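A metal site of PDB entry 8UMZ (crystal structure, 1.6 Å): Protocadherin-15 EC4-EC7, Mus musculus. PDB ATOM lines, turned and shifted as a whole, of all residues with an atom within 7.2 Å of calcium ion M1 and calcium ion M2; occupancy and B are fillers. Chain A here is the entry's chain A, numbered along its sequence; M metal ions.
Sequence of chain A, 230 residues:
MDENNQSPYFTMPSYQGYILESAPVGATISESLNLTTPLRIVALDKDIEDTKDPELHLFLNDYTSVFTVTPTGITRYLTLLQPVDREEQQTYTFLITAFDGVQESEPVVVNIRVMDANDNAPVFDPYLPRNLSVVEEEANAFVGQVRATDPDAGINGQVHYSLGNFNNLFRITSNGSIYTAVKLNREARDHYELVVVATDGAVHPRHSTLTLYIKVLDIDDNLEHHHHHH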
ATOM      1  N   GLU A  21      29.653 -15.719  -9.974  1.00  0.00           N
ATOM      2  CA  GLU A  21      29.444 -16.962 -10.697  1.00  0.00           C
ATOM      3  C   GLU A  21      29.185 -16.703 -12.197  1.00  0.00           C
ATOM      4  O   GLU A  21      29.408 -17.568 -13.026  1.00  0.00           O
ATOM      5  CB  GLU A  21      28.274 -17.804 -10.169  1.00  0.00           C
ATOM      6  CG  GLU A  21      26.891 -17.126 -10.199  1.00  0.00           C
ATOM      7  CD  GLU A  21      25.870 -18.029  -9.545  1.00  0.00           C
ATOM      8  OE1 GLU A  21      25.949 -19.200  -9.750  1.00  0.00           O
ATOM      9  OE2 GLU A  21      24.886 -17.521  -8.864  1.00  0.00           O
ATOM     10  N   ASP A  85      29.423 -22.201 -10.523  1.00  0.00           N
ATOM     11  CA  ASP A  85      28.004 -22.135 -10.214  1.00  0.00           C
ATOM     12  C   ASP A  85      27.838 -22.153  -8.713  1.00  0.00           C
ATOM     13  O   ASP A  85      28.112 -23.158  -8.078  1.00  0.00           O
ATOM     14  CB  ASP A  85      27.299 -23.293 -10.928  1.00  0.00           C
ATOM     15  CG  ASP A  85      25.815 -23.390 -10.589  1.00  0.00           C
ATOM     16  OD1 ASP A  85      25.274 -22.417 -10.097  1.00  0.00           O
ATOM     17  OD2 ASP A  85      25.238 -24.412 -10.827  1.00  0.00           O
ATOM     18  N   ARG A  86      27.221 -21.089  -8.154  1.00  0.00           N
ATOM     19  CA  ARG A  86      27.141 -20.961  -6.733  1.00  0.00           C
ATOM     20  C   ARG A  86      26.133 -21.995  -6.236  1.00  0.00           C
ATOM     21  O   ARG A  86      26.299 -22.512  -5.148  1.00  0.00           O
ATOM     22  CB  ARG A  86      26.808 -19.520  -6.357  1.00  0.00           C
ATOM     23  CG  ARG A  86      26.927 -19.289  -4.858  1.00  0.00           C
ATOM     24  CD  ARG A  86      25.953 -18.210  -4.458  1.00  0.00           C
ATOM     25  NE  ARG A  86      24.578 -18.663  -4.599  1.00  0.00           N
ATOM     26  CZ  ARG A  86      23.951 -19.520  -3.800  1.00  0.00           C
ATOM     27  NH1 ARG A  86      24.550 -20.043  -2.746  1.00  0.00           N
ATOM     28  NH2 ARG A  86      22.690 -19.827  -4.054  1.00  0.00           N
ATOM     29  N   GLU A  87      25.157 -22.360  -7.090  1.00  0.00           N
ATOM     30  CA  GLU A  87      24.120 -23.279  -6.646  1.00  0.00           C
ATOM     31  C   GLU A  87      24.644 -24.728  -6.625  1.00  0.00           C
ATOM     32  O   GLU A  87      24.025 -25.598  -6.018  1.00  0.00           O
ATOM     33  CB  GLU A  87      22.906 -23.186  -7.568  1.00  0.00           C
ATOM     34  CG  GLU A  87      22.018 -21.976  -7.295  1.00  0.00           C
ATOM     35  CD  GLU A  87      22.570 -20.617  -7.668  1.00  0.00           C
ATOM     36  OE1 GLU A  87      22.908 -20.422  -8.845  1.00  0.00           O
ATOM     37  OE2 GLU A  87      22.612 -19.718  -6.769  1.00  0.00           O
ATOM     38  N   MET A 115      30.526 -15.617  -5.513  1.00  0.00           N
ATOM     39  CA  MET A 115      29.458 -14.688  -5.164  1.00  0.00           C
ATOM     40  C   MET A 115      28.224 -14.998  -5.999  1.00  0.00           C
ATOM     41  O   MET A 115      28.316 -15.495  -7.118  1.00  0.00           O
ATOM     42  CB  MET A 115      29.847 -13.225  -5.351  1.00  0.00           C
ATOM     43  CG  MET A 115      31.113 -12.786  -4.628  1.00  0.00           C
ATOM     44  SD  MET A 115      31.042 -13.024  -2.844  1.00  0.00           S
ATOM     45  CE  MET A 115      29.931 -11.684  -2.394  1.00  0.00           C
ATOM     46  N   ASP A 116      27.048 -14.737  -5.426  1.00  0.00           N
ATOM     47  CA  ASP A 116      25.811 -15.057  -6.107  1.00  0.00           C
ATOM     48  C   ASP A 116      25.444 -13.984  -7.107  1.00  0.00           C
ATOM     49  O   ASP A 116      25.466 -12.772  -6.858  1.00  0.00           O
ATOM     50  CB  ASP A 116      24.715 -15.229  -5.058  1.00  0.00           C
ATOM     51  CG  ASP A 116      23.419 -15.727  -5.659  1.00  0.00           C
ATOM     52  OD1 ASP A 116      23.449 -16.729  -6.348  1.00  0.00           O
ATOM     53  OD2 ASP A 116      22.356 -15.088  -5.351  1.00  0.00           O
ATOM     54  N   ALA A 117      25.045 -14.455  -8.281  1.00  0.00           N
ATOM     55  CA  ALA A 117      24.380 -13.646  -9.265  1.00  0.00           C
ATOM     56  C   ALA A 117      22.892 -14.010  -9.164  1.00  0.00           C
ATOM     57  O   ALA A 117      22.549 -15.137  -8.824  1.00  0.00           O
ATOM     58  CB  ALA A 117      24.899 -13.982 -10.643  1.00  0.00           C
ATOM     59  N   ASN A 118      22.024 -13.052  -9.478  1.00  0.00           N
ATOM     60  CA  ASN A 118      20.620 -13.389  -9.663  1.00  0.00           C
ATOM     61  C   ASN A 118      20.386 -13.998 -11.037  1.00  0.00           C
ATOM     62  O   ASN A 118      19.779 -13.340 -11.896  1.00  0.00           O
ATOM     63  CB  ASN A 118      19.713 -12.181  -9.439  1.00  0.00           C
ATOM     64  CG  ASN A 118      18.302 -12.679  -9.388  1.00  0.00           C
ATOM     65  OD1 ASN A 118      18.071 -13.771  -8.882  1.00  0.00           O
ATOM     66  ND2 ASN A 118      17.403 -11.943 -10.034  1.00  0.00           N
ATOM     67  N   ASP A 119      20.820 -15.251 -11.217  1.00  0.00           N
ATOM     68  CA  ASP A 119      20.903 -15.956 -12.499  1.00  0.00           C
ATOM     69  C   ASP A 119      19.774 -16.973 -12.681  1.00  0.00           C
ATOM     70  O   ASP A 119      19.705 -17.725 -13.668  1.00  0.00           O
ATOM     71  CB  ASP A 119      22.311 -16.545 -12.737  1.00  0.00           C
ATOM     72  CG  ASP A 119      22.827 -17.581 -11.747  1.00  0.00           C
ATOM     73  OD1 ASP A 119      22.289 -17.633 -10.630  1.00  0.00           O
ATOM     74  OD2 ASP A 119      23.752 -18.424 -12.114  1.00  0.00           O
ATOM     75  N   ASN A 120      18.830 -16.979 -11.731  1.00  0.00           N
ATOM     76  CA  ASN A 120      17.717 -17.909 -11.775  1.00  0.00           C
ATOM     77  C   ASN A 120      16.430 -17.100 -11.599  1.00  0.00           C
ATOM     78  O   ASN A 120      16.375 -16.188 -10.774  1.00  0.00           O
ATOM     79  CB  ASN A 120      17.795 -19.054 -10.765  1.00  0.00           C
ATOM     80  CG  ASN A 120      18.960 -19.976 -11.055  1.00  0.00           C
ATOM     81  OD1 ASN A 120      20.050 -19.763 -10.547  1.00  0.00           O
ATOM     82  ND2 ASN A 120      18.685 -21.049 -11.764  1.00  0.00           N
ATOM     83  N   ALA A 121      15.424 -17.452 -12.391  1.00  0.00           N
ATOM     84  CA  ALA A 121      14.072 -17.003 -12.140  1.00  0.00           C
ATOM     85  C   ALA A 121      13.383 -17.990 -11.205  1.00  0.00           C
ATOM     86  O   ALA A 121      13.726 -19.156 -11.154  1.00  0.00           O
ATOM     87  CB  ALA A 121      13.325 -16.852 -13.453  1.00  0.00           C
ATOM     88  N   PRO A 122      12.301 -17.593 -10.488  1.00  0.00           N
ATOM     89  CA  PRO A 122      11.502 -18.561  -9.757  1.00  0.00           C
ATOM     90  C   PRO A 122      10.981 -19.630 -10.726  1.00  0.00           C
ATOM     91  O   PRO A 122      10.637 -19.349 -11.874  1.00  0.00           O
ATOM     92  CB  PRO A 122      10.363 -17.671  -9.203  1.00  0.00           C
ATOM     93  CG  PRO A 122      10.987 -16.342  -9.031  1.00  0.00           C
ATOM     94  CD  PRO A 122      11.834 -16.207 -10.273  1.00  0.00           C
ATOM     95  N   ASP A 150      13.125 -20.530  -5.875  1.00  0.00           N
ATOM     96  CA  ASP A 150      14.210 -19.878  -6.582  1.00  0.00           C
ATOM     97  C   ASP A 150      15.473 -20.264  -5.848  1.00  0.00           C
ATOM     98  O   ASP A 150      15.609 -19.963  -4.655  1.00  0.00           O
ATOM     99  CB  ASP A 150      13.982 -18.369  -6.529  1.00  0.00           C
ATOM    100  CG  ASP A 150      14.915 -17.513  -7.370  1.00  0.00           C
ATOM    101  OD1 ASP A 150      16.160 -17.757  -7.354  1.00  0.00           O
ATOM    102  OD2 ASP A 150      14.420 -16.617  -8.029  1.00  0.00           O
ATOM    103  N   PRO A 151      16.439 -20.905  -6.541  1.00  0.00           N
ATOM    104  CA  PRO A 151      17.610 -21.473  -5.864  1.00  0.00           C
ATOM    105  C   PRO A 151      18.679 -20.417  -5.529  1.00  0.00           C
ATOM    106  O   PRO A 151      19.683 -20.801  -4.870  1.00  0.00           O
ATOM    107  CB  PRO A 151      18.068 -22.532  -6.894  1.00  0.00           C
ATOM    108  CG  PRO A 151      17.774 -21.875  -8.221  1.00  0.00           C
ATOM    109  CD  PRO A 151      16.497 -21.068  -7.995  1.00  0.00           C
ATOM    110  N   ASP A 152      18.543 -19.141  -5.982  1.00  0.00           N
ATOM    111  CA  ASP A 152      19.544 -18.121  -5.686  1.00  0.00           C
ATOM    112  C   ASP A 152      19.557 -17.765  -4.203  1.00  0.00           C
ATOM    113  O   ASP A 152      18.725 -18.246  -3.444  1.00  0.00           O
ATOM    114  CB  ASP A 152      19.414 -16.852  -6.524  1.00  0.00           C
ATOM    115  CG  ASP A 152      19.430 -17.084  -8.016  1.00  0.00           C
ATOM    116  OD1 ASP A 152      20.388 -17.675  -8.481  1.00  0.00           O
ATOM    117  OD2 ASP A 152      18.581 -16.494  -8.708  1.00  0.00           O
ATOM    118  N   ALA A 153      20.531 -16.938  -3.807  1.00  0.00           N
ATOM    119  CA  ALA A 153      20.799 -16.634  -2.415  1.00  0.00           C
ATOM    120  C   ALA A 153      20.091 -15.367  -1.966  1.00  0.00           C
ATOM    121  O   ALA A 153      20.027 -14.355  -2.664  1.00  0.00           O
ATOM    122  CB  ALA A 153      22.294 -16.442  -2.220  1.00  0.00           C
ATOM    123  N   ILE A 155      17.986 -12.430  -1.061  1.00  0.00           N
ATOM    124  CA  ILE A 155      16.827 -11.750  -1.683  1.00  0.00           C
ATOM    125  C   ILE A 155      16.672 -12.259  -3.110  1.00  0.00           C
ATOM    126  O   ILE A 155      15.562 -12.351  -3.662  1.00  0.00           O
ATOM    127  CB  ILE A 155      16.952 -10.232  -1.699  1.00  0.00           C
ATOM    128  CG1 ILE A 155      18.197  -9.768  -2.509  1.00  0.00           C
ATOM    129  CG2 ILE A 155      16.893  -9.621  -0.335  1.00  0.00           C
ATOM    130  CD1 ILE A 155      18.448  -8.278  -2.381  1.00  0.00           C
ATOM    131  N   ASN A 156      17.782 -12.721  -3.709  1.00  0.00           N
ATOM    132  CA  ASN A 156      17.727 -13.210  -5.078  1.00  0.00           C
ATOM    133  C   ASN A 156      16.914 -14.512  -5.173  1.00  0.00           C
ATOM    134  O   ASN A 156      16.534 -14.856  -6.274  1.00  0.00           O
ATOM    135  CB  ASN A 156      19.142 -13.370  -5.679  1.00  0.00           C
ATOM    136  CG  ASN A 156      19.983 -12.120  -5.701  1.00  0.00           C
ATOM    137  OD1 ASN A 156      19.472 -10.988  -5.721  1.00  0.00           O
ATOM    138  ND2 ASN A 156      21.317 -12.302  -5.713  1.00  0.00           N
ATOM    139  N   GLY A 157      16.696 -15.223  -4.050  1.00  0.00           N
ATOM    140  CA  GLY A 157      15.963 -16.473  -3.988  1.00  0.00           C
ATOM    141  C   GLY A 157      14.624 -16.331  -3.250  1.00  0.00           C
ATOM    142  O   GLY A 157      13.932 -17.325  -3.156  1.00  0.00           O
ATOM    143  N   GLN A 158      14.250 -15.116  -2.818  1.00  0.00           N
ATOM    144  CA  GLN A 158      12.955 -14.904  -2.155  1.00  0.00           C
ATOM    145  C   GLN A 158      11.883 -14.550  -3.168  1.00  0.00           C
ATOM    146  O   GLN A 158      12.088 -13.762  -4.087  1.00  0.00           O
ATOM    147  CB  GLN A 158      13.061 -13.878  -1.047  1.00  0.00           C
ATOM    148  CG  GLN A 158      13.874 -14.388   0.125  1.00  0.00           C
ATOM    149  CD  GLN A 158      14.225 -13.239   1.038  1.00  0.00           C
ATOM    150  OE1 GLN A 158      13.643 -12.139   1.031  1.00  0.00           O
ATOM    151  NE2 GLN A 158      15.275 -13.446   1.800  1.00  0.00           N
ATOM    152  N   THR A 199       7.993 -13.389  -8.656  1.00  0.00           N
ATOM    153  CA  THR A 199       9.098 -12.426  -8.839  1.00  0.00           C
ATOM    154  C   THR A 199      10.044 -12.570  -7.649  1.00  0.00           C
ATOM    155  O   THR A 199       9.633 -12.692  -6.505  1.00  0.00           O
ATOM    156  CB  THR A 199       8.578 -10.999  -8.887  1.00  0.00           C
ATOM    157  OG1 THR A 199       7.588 -10.854  -9.931  1.00  0.00           O
ATOM    158  CG2 THR A 199       9.670  -9.967  -9.089  1.00  0.00           C
ATOM    159  N   ASP A 200      11.356 -12.649  -7.905  1.00  0.00           N
ATOM    160  CA  ASP A 200      12.286 -12.640  -6.785  1.00  0.00           C
ATOM    161  C   ASP A 200      12.514 -11.235  -6.228  1.00  0.00           C
ATOM    162  O   ASP A 200      12.026 -10.234  -6.749  1.00  0.00           O
ATOM    163  CB  ASP A 200      13.553 -13.408  -7.167  1.00  0.00           C
ATOM    164  CG  ASP A 200      14.341 -12.863  -8.346  1.00  0.00           C
ATOM    165  OD1 ASP A 200      14.328 -11.667  -8.487  1.00  0.00           O
ATOM    166  OD2 ASP A 200      15.017 -13.714  -9.092  1.00  0.00           O
ATOM    167  N   GLY A 201      13.282 -11.192  -5.116  1.00  0.00           N
ATOM    168  CA  GLY A 201      13.607  -9.982  -4.390  1.00  0.00           C
ATOM    169  C   GLY A 201      14.890  -9.280  -4.841  1.00  0.00           C
ATOM    170  O   GLY A 201      15.281  -8.334  -4.188  1.00  0.00           O
ATOM    171  N   ALA A 202      15.469  -9.611  -5.982  1.00  0.00           N
ATOM    172  CA  ALA A 202      16.735  -9.024  -6.384  1.00  0.00           C
ATOM    173  C   ALA A 202      16.614  -7.539  -6.695  1.00  0.00           C
ATOM    174  O   ALA A 202      15.554  -7.037  -7.090  1.00  0.00           O
ATOM    175  CB  ALA A 202      17.240  -9.761  -7.564  1.00  0.00           C
ATOM    176  N   HIS A 204      17.872  -6.410  -9.310  1.00  0.00           N
ATOM    177  CA  HIS A 204      17.535  -6.526 -10.720  1.00  0.00           C
ATOM    178  C   HIS A 204      16.617  -7.745 -10.806  1.00  0.00           C
ATOM    179  O   HIS A 204      17.113  -8.847 -10.992  1.00  0.00           O
ATOM    180  CB  HIS A 204      18.831  -6.651 -11.537  1.00  0.00           C
ATOM    181  CG  HIS A 204      19.792  -5.516 -11.364  1.00  0.00           C
ATOM    182  ND1 HIS A 204      21.080  -5.689 -10.885  1.00  0.00           N
ATOM    183  CD2 HIS A 204      19.666  -4.197 -11.631  1.00  0.00           C
ATOM    184  CE1 HIS A 204      21.685  -4.494 -10.866  1.00  0.00           C
ATOM    185  NE2 HIS A 204      20.862  -3.595 -11.339  1.00  0.00           N
ATOM    186  N   PRO A 205      15.301  -7.620 -10.515  1.00  0.00           N
ATOM    187  CA  PRO A 205      14.469  -8.814 -10.287  1.00  0.00           C
ATOM    188  C   PRO A 205      14.328  -9.689 -11.514  1.00  0.00           C
ATOM    189  O   PRO A 205      14.399  -9.194 -12.643  1.00  0.00           O
ATOM    190  CB  PRO A 205      13.130  -8.209  -9.856  1.00  0.00           C
ATOM    191  CG  PRO A 205      13.155  -6.835 -10.471  1.00  0.00           C
ATOM    192  CD  PRO A 205      14.580  -6.392 -10.191  1.00  0.00           C
ATOM    193  N   ARG A 206      14.085 -10.978 -11.294  1.00  0.00           N
ATOM    194  CA  ARG A 206      13.680 -11.900 -12.365  1.00  0.00           C
ATOM    195  C   ARG A 206      12.290 -12.427 -11.998  1.00  0.00           C
ATOM    196  O   ARG A 206      11.949 -12.468 -10.811  1.00  0.00           O
ATOM    197  CB  ARG A 206      14.657 -13.040 -12.585  1.00  0.00           C
ATOM    198  CG  ARG A 206      15.968 -12.643 -13.251  1.00  0.00           C
ATOM    199  CD  ARG A 206      16.795 -13.881 -13.503  1.00  0.00           C
ATOM    200  NE  ARG A 206      18.067 -13.628 -14.206  1.00  0.00           N
ATOM    201  CZ  ARG A 206      18.164 -13.473 -15.535  1.00  0.00           C
ATOM    202  NH1 ARG A 206      17.081 -13.503 -16.292  1.00  0.00           N
ATOM    203  NH2 ARG A 206      19.340 -13.234 -16.115  1.00  0.00           N
HETATM  204 CA    CA M   1      22.713 -17.613  -8.363  1.00  0.00          CA
HETATM  205 CA    CA M   2      16.501 -15.488  -8.518  1.00  0.00          CA
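Six residues have an atom within 4 Å of calcium ion M1: Glu 21, Glu 87, Asp 116, Ala 117, Asp 119 and Asp 152. Along chain A the residues within 4 Å of calcium ion M1 span positions 21 to 152. The nearest printed residue that does not touch calcium ion M1 is Asn 120 (4.1 Å).
The side-chain carboxylate (OE2) of Glu 21 binds calcium ion M1 (2.2 Å). Calcium ion M1 is bound by OD1 of Asp 119 (2.3 Å). The side-chain carboxylate (OD1) of Asp 116 is bound to calcium ion M1 (2.3 Å). Calcium ion M1 is bound by OD1 of Asp 152 (2.3 Å). Calcium ion M1 is bound by O of Ala 117 (2.5 Å). The side-chain carboxylate (OE2) of Glu 87 is bound to calcium ion M1 (2.6 Å). OE1 of Glu 87 binds calcium ion M1, at 2.9 Å. Calcium ion M1 has seven donor atoms within binding distance.
The side-chain amide oxygen of Asn 120 lies close to the side-chain carboxylate of Glu 87 (3.4 Å). OE1 of Glu 21 lies within hydrogen-bond range of N of Arg 86. The guanidinium group (NE) of Arg 86 lies close to the side-chain carboxylate (OD1) of Asp 116 (2.8 Å). The backbone NH (N) of Glu 87 sits at hydrogen-bond distance from the side-chain carboxylate (OD1) of Asp 85, 3.0 Å away. The side-chain carboxylate (OD1) of Asp 200 sits at hydrogen-bond distance from the backbone NH (N) of Arg 206. OD1 of Asp 200 sits close to N of Ala 202 (3.4 Å). OD2 of Asp 116 sits at hydrogen-bond distance from N of Ala 153, 3.0 Å away. The side-chain carboxylate (OE2) of Glu 87 lies close to the guanidinium group (NH2) of Arg 86, at 2.7 Å.
The side-chain carboxylate (OD2) of Asp 152 is bound to calcium ion M2, at 2.3 Å. O of Asn 156 binds calcium ion M2, at 2.3 Å. OD1 of Asn 118 is bound to calcium ion M2 (2.4 Å). Calcium ion M2 is bound by the backbone carbonyl oxygen (O) of Asn 120. The side-chain carboxylate (OD2) of Asp 200 is bound to calcium ion M2 (2.4 Å). OD2 of Asp 150 binds calcium ion M2, at 2.4 Å. Calcium ion M2 is bound by OD1 of Asp 150 (2.6 Å).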
